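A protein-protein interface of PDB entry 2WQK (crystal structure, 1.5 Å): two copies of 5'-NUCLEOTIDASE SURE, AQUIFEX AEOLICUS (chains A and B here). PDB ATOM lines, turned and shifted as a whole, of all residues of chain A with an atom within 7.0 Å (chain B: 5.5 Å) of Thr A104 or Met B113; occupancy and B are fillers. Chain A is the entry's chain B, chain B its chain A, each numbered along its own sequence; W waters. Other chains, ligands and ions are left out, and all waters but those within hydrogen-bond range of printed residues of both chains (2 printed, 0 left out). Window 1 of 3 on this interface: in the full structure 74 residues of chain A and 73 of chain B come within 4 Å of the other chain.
Of the printed residues of chain B, Glu A101 touches Ile B117 (3.4 Å). Printed residues of chain B within 4 Å of Thr A104: Thr B104 (3.7 Å) and Met B113 (3.5 Å). Val A109 touches none of the printed residues of chain B. Of the printed residues of chain B, Arg A183 touches Glu B114 (2.8 Å) and Ile B117 (3.7 Å). Of the printed residues of chain A, Ser B110 touches Tyr A105. Of the printed residues of chain A, Met B113 touches Thr A104 and Tyr A105. Tyr B159 touches none of the printed residues of chain A. The nearest printed residue of chain B that does not touch Thr A104 is Leu B235 (4.2 Å). The nearest printed residue of chain A that does not touch Leu B235 is Thr A104 (4.2 Å).
Thr B104 touches its own counterpart, Thr A104. 3 positions are printed for both chains.
A ring nitrogen (ND1) of His A44 lies close to the backbone carbonyl oxygen of Tyr A105 (3.4 Å). O of Gly A100 lies within hydrogen-bond range of NE2 of Gln A180 (2.9 Å). The backbone NH (N) of Arg A183 lies within hydrogen-bond range of the side-chain carboxylate (OE1) of Glu A101 (3.3 Å). OD1 of Asp A102 lies within salt-bridge range of NH2 of Arg A183, 2.9 Å away.
Water W1 lies within hydrogen-bond range of the backbone carbonyl oxygen of Ile B117 (2.9 Å) and the side-chain carboxylate of Glu A101 (2.9 Å). Water W2 lies within hydrogen-bond range of the side-chain amide nitrogen of Gln A180, the backbone carbonyl oxygen of Leu B233 and the side-chain hydroxyl of Thr A104.
Glu A101 touches Ile B117 (OE1 to CG2, 3.4 Å). Ile A103 touches Leu B235. O of Thr A104 touches O of Thr B104 (3.7 Å). Tyr A105 touches Ser B110. CE of Met B113 touches OH of Tyr A105, at 3.4 Å. OE1 of Gln A180 touches O of Leu B233 (3.9 Å). Arg A183 touches Ile B117 (NH1 to CG2, 3.7 Å).
Of the 14 printed residues of chain A, 6 touch a printed residue of chain B. Printed residues of chain A that touch a printed residue of chain B: Glu A101, Ile A103, Thr A104, Tyr A105, Gln A180 and Arg A183. Hydrophobic or aromatic side chains of chain A within 4 Å of the printed part of chain B: Ile A103 and Tyr A105. Along chain A the printed residues that touch a printed residue of chain B span positions 101 to 183. Printed residues of chain B that touch a printed residue of chain A: Thr B104, Ser B110, Met B113, Glu B114, Ile B117, Leu B233 and Leu B235. Hydrophobic or aromatic side chains of chain B that line the printed part of chain A: Met B113, Ile B117 and Leu B235.
The side-chain hydroxyl of Thr A104 sits at hydrogen-bond distance from the side-chain sulfur of Met B113. OE2 of Glu B114 is in hydrogen-bond range of OH of Tyr A105. The side-chain carboxylate of Glu B114 lies within salt-bridge range of the guanidinium group of Arg A183 (2.8 Å). N of Leu B235 sits at hydrogen-bond distance from OE1 of Gln A180.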
ATOM      1  N   HIS A  44     -29.029  20.346  24.749  1.00  0.00           N
ATOM      2  CA  HIS A  44     -28.967  20.785  23.361  1.00  0.00           C
ATOM      3  C   HIS A  44     -28.740  19.668  22.360  1.00  0.00           C
ATOM      4  O   HIS A  44     -28.591  19.927  21.181  1.00  0.00           O
ATOM      5  CB  HIS A  44     -27.838  21.816  23.241  1.00  0.00           C
ATOM      6  CG  HIS A  44     -28.027  22.993  24.123  1.00  0.00           C
ATOM      7  ND1 HIS A  44     -26.996  23.593  24.818  1.00  0.00           N
ATOM      8  CD2 HIS A  44     -29.152  23.666  24.456  1.00  0.00           C
ATOM      9  CE1 HIS A  44     -27.480  24.600  25.525  1.00  0.00           C
ATOM     10  NE2 HIS A  44     -28.784  24.673  25.321  1.00  0.00           N
ATOM     11  N   LEU A  99     -18.554  33.160  24.724  1.00  0.00           N
ATOM     12  CA  LEU A  99     -17.146  33.431  24.652  1.00  0.00           C
ATOM     13  C   LEU A  99     -16.361  32.374  25.443  1.00  0.00           C
ATOM     14  O   LEU A  99     -16.876  31.777  26.403  1.00  0.00           O
ATOM     15  CB  LEU A  99     -16.887  34.803  25.319  1.00  0.00           C
ATOM     16  CG  LEU A  99     -17.512  35.979  24.585  1.00  0.00           C
ATOM     17  CD1 LEU A  99     -17.647  37.205  25.543  1.00  0.00           C
ATOM     18  CD2 LEU A  99     -16.725  36.347  23.338  1.00  0.00           C
ATOM     19  N   GLY A 100     -15.121  32.206  25.038  1.00  0.00           N
ATOM     20  CA  GLY A 100     -14.171  31.461  25.843  1.00  0.00           C
ATOM     21  C   GLY A 100     -14.608  30.034  26.064  1.00  0.00           C
ATOM     22  O   GLY A 100     -15.220  29.385  25.213  1.00  0.00           O
ATOM     23  N   GLU A 101     -14.337  29.577  27.278  1.00  0.00           N
ATOM     24  CA  GLU A 101     -14.526  28.189  27.616  1.00  0.00           C
ATOM     25  C   GLU A 101     -16.027  27.805  27.659  1.00  0.00           C
ATOM     26  O   GLU A 101     -16.398  26.622  27.522  1.00  0.00           O
ATOM     27  CB  GLU A 101     -13.668  27.852  28.904  1.00  0.00           C
ATOM     28  CG  GLU A 101     -12.148  27.570  28.583  1.00  0.00           C
ATOM     29  CD  GLU A 101     -11.118  27.984  29.663  1.00  0.00           C
ATOM     30  OE1 GLU A 101     -11.490  28.614  30.652  1.00  0.00           O
ATOM     31  OE2 GLU A 101      -9.906  27.675  29.510  1.00  0.00           O
ATOM     32  N   ASP A 102     -16.912  28.793  27.766  1.00  0.00           N
ATOM     33  CA  ASP A 102     -18.352  28.555  27.809  1.00  0.00           C
ATOM     34  C   ASP A 102     -19.002  28.163  26.434  1.00  0.00           C
ATOM     35  O   ASP A 102     -20.171  27.726  26.325  1.00  0.00           O
ATOM     36  CB  ASP A 102     -18.974  29.710  28.595  1.00  0.00           C
ATOM     37  CG  ASP A 102     -18.451  29.729  30.072  1.00  0.00           C
ATOM     38  OD1 ASP A 102     -18.362  28.634  30.699  1.00  0.00           O
ATOM     39  OD2 ASP A 102     -18.067  30.801  30.585  1.00  0.00           O
ATOM     40  N   ILE A 103     -18.198  28.255  25.393  1.00  0.00           N
ATOM     41  CA  ILE A 103     -18.666  27.876  24.034  1.00  0.00           C
ATOM     42  C   ILE A 103     -19.176  26.418  23.989  1.00  0.00           C
ATOM     43  O   ILE A 103     -20.156  26.109  23.334  1.00  0.00           O
ATOM     44  CB  ILE A 103     -17.539  28.092  23.001  1.00  0.00           C
ATOM     45  CG1 ILE A 103     -17.300  29.592  22.759  1.00  0.00           C
ATOM     46  CG2 ILE A 103     -17.804  27.383  21.683  1.00  0.00           C
ATOM     47  CD1 ILE A 103     -15.931  29.885  22.074  1.00  0.00           C
ATOM     48  N   THR A 104     -18.505  25.531  24.722  1.00  0.00           N
ATOM     49  CA  THR A 104     -18.854  24.116  24.748  1.00  0.00           C
ATOM     50  C   THR A 104     -20.291  23.852  25.171  1.00  0.00           C
ATOM     51  O   THR A 104     -20.891  22.870  24.788  1.00  0.00           O
ATOM     52  CB  THR A 104     -17.942  23.361  25.739  1.00  0.00           C
ATOM     53  OG1 THR A 104     -16.593  23.419  25.248  1.00  0.00           O
ATOM     54  CG2 THR A 104     -18.410  21.922  25.916  1.00  0.00           C
ATOM     55  N   TYR A 105     -20.842  24.727  26.011  1.00  0.00           N
ATOM     56  CA  TYR A 105     -22.163  24.559  26.588  1.00  0.00           C
ATOM     57  C   TYR A 105     -23.272  25.321  25.832  1.00  0.00           C
ATOM     58  O   TYR A 105     -24.450  25.284  26.193  1.00  0.00           O
ATOM     59  CB  TYR A 105     -22.182  25.042  28.053  1.00  0.00           C
ATOM     60  CG  TYR A 105     -21.184  24.325  28.948  1.00  0.00           C
ATOM     61  CD1 TYR A 105     -21.350  23.008  29.227  1.00  0.00           C
ATOM     62  CD2 TYR A 105     -20.090  24.953  29.458  1.00  0.00           C
ATOM     63  CE1 TYR A 105     -20.449  22.339  30.024  1.00  0.00           C
ATOM     64  CE2 TYR A 105     -19.181  24.289  30.274  1.00  0.00           C
ATOM     65  CZ  TYR A 105     -19.378  22.968  30.563  1.00  0.00           C
ATOM     66  OH  TYR A 105     -18.480  22.276  31.380  1.00  0.00           O
ATOM     67  N   SER A 106     -22.893  26.018  24.789  1.00  0.00           N
ATOM     68  CA  SER A 106     -23.851  26.907  24.088  1.00  0.00           C
ATOM     69  C   SER A 106     -24.709  26.201  23.043  1.00  0.00           C
ATOM     70  O   SER A 106     -24.181  25.582  22.115  1.00  0.00           O
ATOM     71  CB  SER A 106     -23.055  27.969  23.356  1.00  0.00           C
ATOM     72  OG  SER A 106     -23.849  28.743  22.463  1.00  0.00           O
ATOM     73  N   GLY A 107     -26.008  26.402  23.146  1.00  0.00           N
ATOM     74  CA  GLY A 107     -26.930  25.927  22.132  1.00  0.00           C
ATOM     75  C   GLY A 107     -26.815  26.707  20.840  1.00  0.00           C
ATOM     76  O   GLY A 107     -27.013  26.153  19.770  1.00  0.00           O
ATOM     77  N   VAL A 109     -24.071  28.013  19.605  1.00  0.00           N
ATOM     78  CA  VAL A 109     -22.873  27.497  18.930  1.00  0.00           C
ATOM     79  C   VAL A 109     -23.142  26.084  18.379  1.00  0.00           C
ATOM     80  O   VAL A 109     -22.754  25.784  17.276  1.00  0.00           O
ATOM     81  CB  VAL A 109     -21.640  27.539  19.852  1.00  0.00           C
ATOM     82  CG1 VAL A 109     -20.447  26.931  19.146  1.00  0.00           C
ATOM     83  CG2 VAL A 109     -21.345  28.957  20.286  1.00  0.00           C
ATOM     84  N   SER A 110     -23.847  25.250  19.141  1.00  0.00           N
ATOM     85  CA  SER A 110     -24.087  23.874  18.693  1.00  0.00           C
ATOM     86  C   SER A 110     -24.937  23.832  17.399  1.00  0.00           C
ATOM     87  O   SER A 110     -24.747  22.957  16.540  1.00  0.00           O
ATOM     88  CB  SER A 110     -24.680  23.039  19.823  1.00  0.00           C
ATOM     89  OG  SER A 110     -25.964  23.390  20.104  1.00  0.00           O
ATOM     90  N   GLN A 180     -10.264  31.653  21.002  1.00  0.00           N
ATOM     91  CA  GLN A 180     -11.075  31.380  22.165  1.00  0.00           C
ATOM     92  C   GLN A 180     -10.269  31.766  23.422  1.00  0.00           C
ATOM     93  O   GLN A 180      -9.190  31.242  23.644  1.00  0.00           O
ATOM     94  CB  GLN A 180     -11.374  29.891  22.228  1.00  0.00           C
ATOM     95  CG  GLN A 180     -12.179  29.441  23.443  1.00  0.00           C
ATOM     96  CD  GLN A 180     -12.340  27.935  23.485  1.00  0.00           C
ATOM     97  OE1 GLN A 180     -11.431  27.215  23.094  1.00  0.00           O
ATOM     98  NE2 GLN A 180     -13.483  27.457  24.023  1.00  0.00           N
ATOM     99  N   ARG A 183     -11.565  31.906  30.629  1.00  0.00           N
ATOM    100  CA  ARG A 183     -12.633  32.657  31.287  1.00  0.00           C
ATOM    101  C   ARG A 183     -12.133  33.972  31.875  1.00  0.00           C
ATOM    102  O   ARG A 183     -11.226  34.001  32.680  1.00  0.00           O
ATOM    103  CB  ARG A 183     -13.289  31.819  32.380  1.00  0.00           C
ATOM    104  CG  ARG A 183     -14.240  30.784  31.812  1.00  0.00           C
ATOM    105  CD  ARG A 183     -14.502  29.683  32.775  1.00  0.00           C
ATOM    106  NE  ARG A 183     -15.518  28.787  32.237  1.00  0.00           N
ATOM    107  CZ  ARG A 183     -15.653  27.499  32.558  1.00  0.00           C
ATOM    108  NH1 ARG A 183     -14.807  26.939  33.408  1.00  0.00           N
ATOM    109  NH2 ARG A 183     -16.592  26.767  31.981  1.00  0.00           N
ATOM    110  N   THR B 104     -19.484  16.664  22.251  1.00  0.00           N
ATOM    111  CA  THR B 104     -19.833  18.048  22.586  1.00  0.00           C
ATOM    112  C   THR B 104     -20.974  18.192  23.575  1.00  0.00           C
ATOM    113  O   THR B 104     -21.049  19.154  24.314  1.00  0.00           O
ATOM    114  CB  THR B 104     -20.255  18.803  21.309  1.00  0.00           C
ATOM    115  OG1 THR B 104     -19.134  18.826  20.418  1.00  0.00           O
ATOM    116  CG2 THR B 104     -20.693  20.196  21.650  1.00  0.00           C
ATOM    117  N   VAL B 109     -17.958  13.989  29.578  1.00  0.00           N
ATOM    118  CA  VAL B 109     -16.793  14.605  28.961  1.00  0.00           C
ATOM    119  C   VAL B 109     -16.556  16.014  29.545  1.00  0.00           C
ATOM    120  O   VAL B 109     -15.440  16.401  29.816  1.00  0.00           O
ATOM    121  CB  VAL B 109     -16.894  14.620  27.416  1.00  0.00           C
ATOM    122  CG1 VAL B 109     -15.691  15.314  26.813  1.00  0.00           C
ATOM    123  CG2 VAL B 109     -16.998  13.208  26.898  1.00  0.00           C
ATOM    124  N   SER B 110     -17.625  16.771  29.745  1.00  0.00           N
ATOM    125  CA  SER B 110     -17.459  18.143  30.239  1.00  0.00           C
ATOM    126  C   SER B 110     -16.854  18.186  31.654  1.00  0.00           C
ATOM    127  O   SER B 110     -16.088  19.116  31.968  1.00  0.00           O
ATOM    128  CB  SER B 110     -18.782  18.911  30.171  1.00  0.00           C
ATOM    129  OG  SER B 110     -19.725  18.446  31.067  1.00  0.00           O
ATOM    130  N   GLY B 111     -17.129  17.158  32.467  1.00  0.00           N
ATOM    131  CA  GLY B 111     -16.456  17.080  33.784  1.00  0.00           C
ATOM    132  C   GLY B 111     -14.938  17.013  33.619  1.00  0.00           C
ATOM    133  O   GLY B 111     -14.182  17.708  34.316  1.00  0.00           O
ATOM    134  N   ALA B 112     -14.467  16.150  32.716  1.00  0.00           N
ATOM    135  CA  ALA B 112     -13.018  16.054  32.468  1.00  0.00           C
ATOM    136  C   ALA B 112     -12.481  17.376  31.873  1.00  0.00           C
ATOM    137  O   ALA B 112     -11.429  17.866  32.261  1.00  0.00           O
ATOM    138  CB  ALA B 112     -12.660  14.871  31.592  1.00  0.00           C
ATOM    139  N   MET B 113     -13.241  17.974  30.951  1.00  0.00           N
ATOM    140  CA  MET B 113     -12.856  19.263  30.399  1.00  0.00           C
ATOM    141  C   MET B 113     -12.639  20.315  31.470  1.00  0.00           C
ATOM    142  O   MET B 113     -11.656  21.011  31.436  1.00  0.00           O
ATOM    143  CB  MET B 113     -13.917  19.731  29.382  1.00  0.00           C
ATOM    144  CG  MET B 113     -13.527  21.016  28.668  1.00  0.00           C
ATOM    145  SD  MET B 113     -14.919  21.740  27.763  1.00  0.00           S
ATOM    146  CE  MET B 113     -15.946  22.251  29.149  1.00  0.00           C
ATOM    147  N   GLU B 114     -13.564  20.368  32.407  1.00  0.00           N
ATOM    148  CA  GLU B 114     -13.469  21.334  33.510  1.00  0.00           C
ATOM    149  C   GLU B 114     -12.214  21.109  34.362  1.00  0.00           C
ATOM    150  O   GLU B 114     -11.550  22.059  34.807  1.00  0.00           O
ATOM    151  CB  GLU B 114     -14.744  21.355  34.353  1.00  0.00           C
ATOM    152  CG  GLU B 114     -15.930  21.897  33.593  1.00  0.00           C
ATOM    153  CD  GLU B 114     -15.862  23.407  33.276  1.00  0.00           C
ATOM    154  OE1 GLU B 114     -15.050  24.147  33.869  1.00  0.00           O
ATOM    155  OE2 GLU B 114     -16.657  23.853  32.415  1.00  0.00           O
ATOM    156  N   GLY B 115     -11.904  19.844  34.607  1.00  0.00           N
ATOM    157  CA  GLY B 115     -10.637  19.585  35.308  1.00  0.00           C
ATOM    158  C   GLY B 115      -9.456  20.174  34.574  1.00  0.00           C
ATOM    159  O   GLY B 115      -8.614  20.836  35.173  1.00  0.00           O
ATOM    160  N   ARG B 116      -9.404  19.975  33.246  1.00  0.00           N
ATOM    161  CA  ARG B 116      -8.276  20.468  32.461  1.00  0.00           C
ATOM    162  C   ARG B 116      -8.295  22.008  32.397  1.00  0.00           C
ATOM    163  O   ARG B 116      -7.235  22.629  32.417  1.00  0.00           O
ATOM    164  CB  ARG B 116      -8.250  19.812  31.061  1.00  0.00           C
ATOM    165  CG  ARG B 116      -6.917  19.882  30.338  1.00  0.00           C
ATOM    166  CD  ARG B 116      -5.670  19.634  31.202  1.00  0.00           C
ATOM    167  NE  ARG B 116      -4.932  20.887  31.462  1.00  0.00           N
ATOM    168  CZ  ARG B 116      -3.851  21.068  32.236  1.00  0.00           C
ATOM    169  NH1 ARG B 116      -3.314  22.276  32.312  1.00  0.00           N
ATOM    170  NH2 ARG B 116      -3.294  20.085  32.921  1.00  0.00           N
ATOM    171  N   ILE B 117      -9.492  22.614  32.399  1.00  0.00           N
ATOM    172  CA  ILE B 117      -9.593  24.104  32.453  1.00  0.00           C
ATOM    173  C   ILE B 117      -8.931  24.620  33.735  1.00  0.00           C
ATOM    174  O   ILE B 117      -8.262  25.678  33.734  1.00  0.00           O
ATOM    175  CB  ILE B 117     -11.049  24.572  32.380  1.00  0.00           C
ATOM    176  CG1 ILE B 117     -11.550  24.395  30.948  1.00  0.00           C
ATOM    177  CG2 ILE B 117     -11.245  26.058  32.836  1.00  0.00           C
ATOM    178  CD1 ILE B 117     -13.059  24.599  30.785  1.00  0.00           C
ATOM    179  N   LEU B 118      -9.107  23.859  34.817  1.00  0.00           N
ATOM    180  CA  LEU B 118      -8.542  24.210  36.107  1.00  0.00           C
ATOM    181  C   LEU B 118      -7.059  23.867  36.227  1.00  0.00           C
ATOM    182  O   LEU B 118      -6.476  24.096  37.306  1.00  0.00           O
ATOM    183  CB  LEU B 118      -9.310  23.493  37.221  1.00  0.00           C
ATOM    184  CG  LEU B 118     -10.710  24.039  37.503  1.00  0.00           C
ATOM    185  CD1 LEU B 118     -11.509  23.191  38.497  1.00  0.00           C
ATOM    186  CD2 LEU B 118     -10.688  25.482  38.011  1.00  0.00           C
ATOM    187  N   SER B 122      -6.814  15.249  33.153  1.00  0.00           N
ATOM    188  CA  SER B 122      -8.185  14.764  33.295  1.00  0.00           C
ATOM    189  C   SER B 122      -8.564  13.713  32.263  1.00  0.00           C
ATOM    190  O   SER B 122      -8.070  13.740  31.146  1.00  0.00           O
ATOM    191  CB  SER B 122      -9.201  15.900  33.298  1.00  0.00           C
ATOM    192  OG  SER B 122      -8.894  16.931  34.224  1.00  0.00           O
ATOM    193  N   TYR B 159      -7.029  16.618  27.048  1.00  0.00           N
ATOM    194  CA  TYR B 159      -7.620  15.722  28.064  1.00  0.00           C
ATOM    195  C   TYR B 159      -8.092  14.483  27.326  1.00  0.00           C
ATOM    196  O   TYR B 159      -8.245  14.522  26.109  1.00  0.00           O
ATOM    197  CB  TYR B 159      -8.699  16.393  28.906  1.00  0.00           C
ATOM    198  CG  TYR B 159      -9.900  16.926  28.138  1.00  0.00           C
ATOM    199  CD1 TYR B 159     -11.125  16.310  28.266  1.00  0.00           C
ATOM    200  CD2 TYR B 159      -9.828  18.072  27.326  1.00  0.00           C
ATOM    201  CE1 TYR B 159     -12.236  16.729  27.565  1.00  0.00           C
ATOM    202  CE2 TYR B 159     -10.952  18.511  26.631  1.00  0.00           C
ATOM    203  CZ  TYR B 159     -12.146  17.844  26.759  1.00  0.00           C
ATOM    204  OH  TYR B 159     -13.266  18.267  26.080  1.00  0.00           O
ATOM    205  N   LEU B 233      -8.346  21.046  24.415  1.00  0.00           N
ATOM    206  CA  LEU B 233      -9.080  21.959  25.256  1.00  0.00           C
ATOM    207  C   LEU B 233      -9.415  23.251  24.474  1.00  0.00           C
ATOM    208  O   LEU B 233     -10.546  23.741  24.518  1.00  0.00           O
ATOM    209  CB  LEU B 233      -8.296  22.342  26.516  1.00  0.00           C
ATOM    210  CG  LEU B 233      -9.140  23.307  27.391  1.00  0.00           C
ATOM    211  CD1 LEU B 233     -10.584  22.817  27.757  1.00  0.00           C
ATOM    212  CD2 LEU B 233      -8.349  23.691  28.632  1.00  0.00           C
ATOM    213  N   LEU B 235     -10.417  25.176  21.372  1.00  0.00           N
ATOM    214  CA  LEU B 235     -11.162  24.880  20.163  1.00  0.00           C
ATOM    215  C   LEU B 235     -10.681  25.698  18.957  1.00  0.00           C
ATOM    216  O   LEU B 235     -11.182  25.494  17.850  1.00  0.00           O
ATOM    217  CB  LEU B 235     -12.679  25.156  20.379  1.00  0.00           C
ATOM    218  CG  LEU B 235     -13.352  24.620  21.632  1.00  0.00           C
ATOM    219  CD1 LEU B 235     -14.841  25.063  21.769  1.00  0.00           C
ATOM    220  CD2 LEU B 235     -13.235  23.125  21.586  1.00  0.00           C
HETATM  221  O   HOH W   1      -7.892  27.516  31.586  1.00  0.00           O
HETATM  222  O   HOH W   2     -13.503  24.755  25.694  1.00  0.00           O
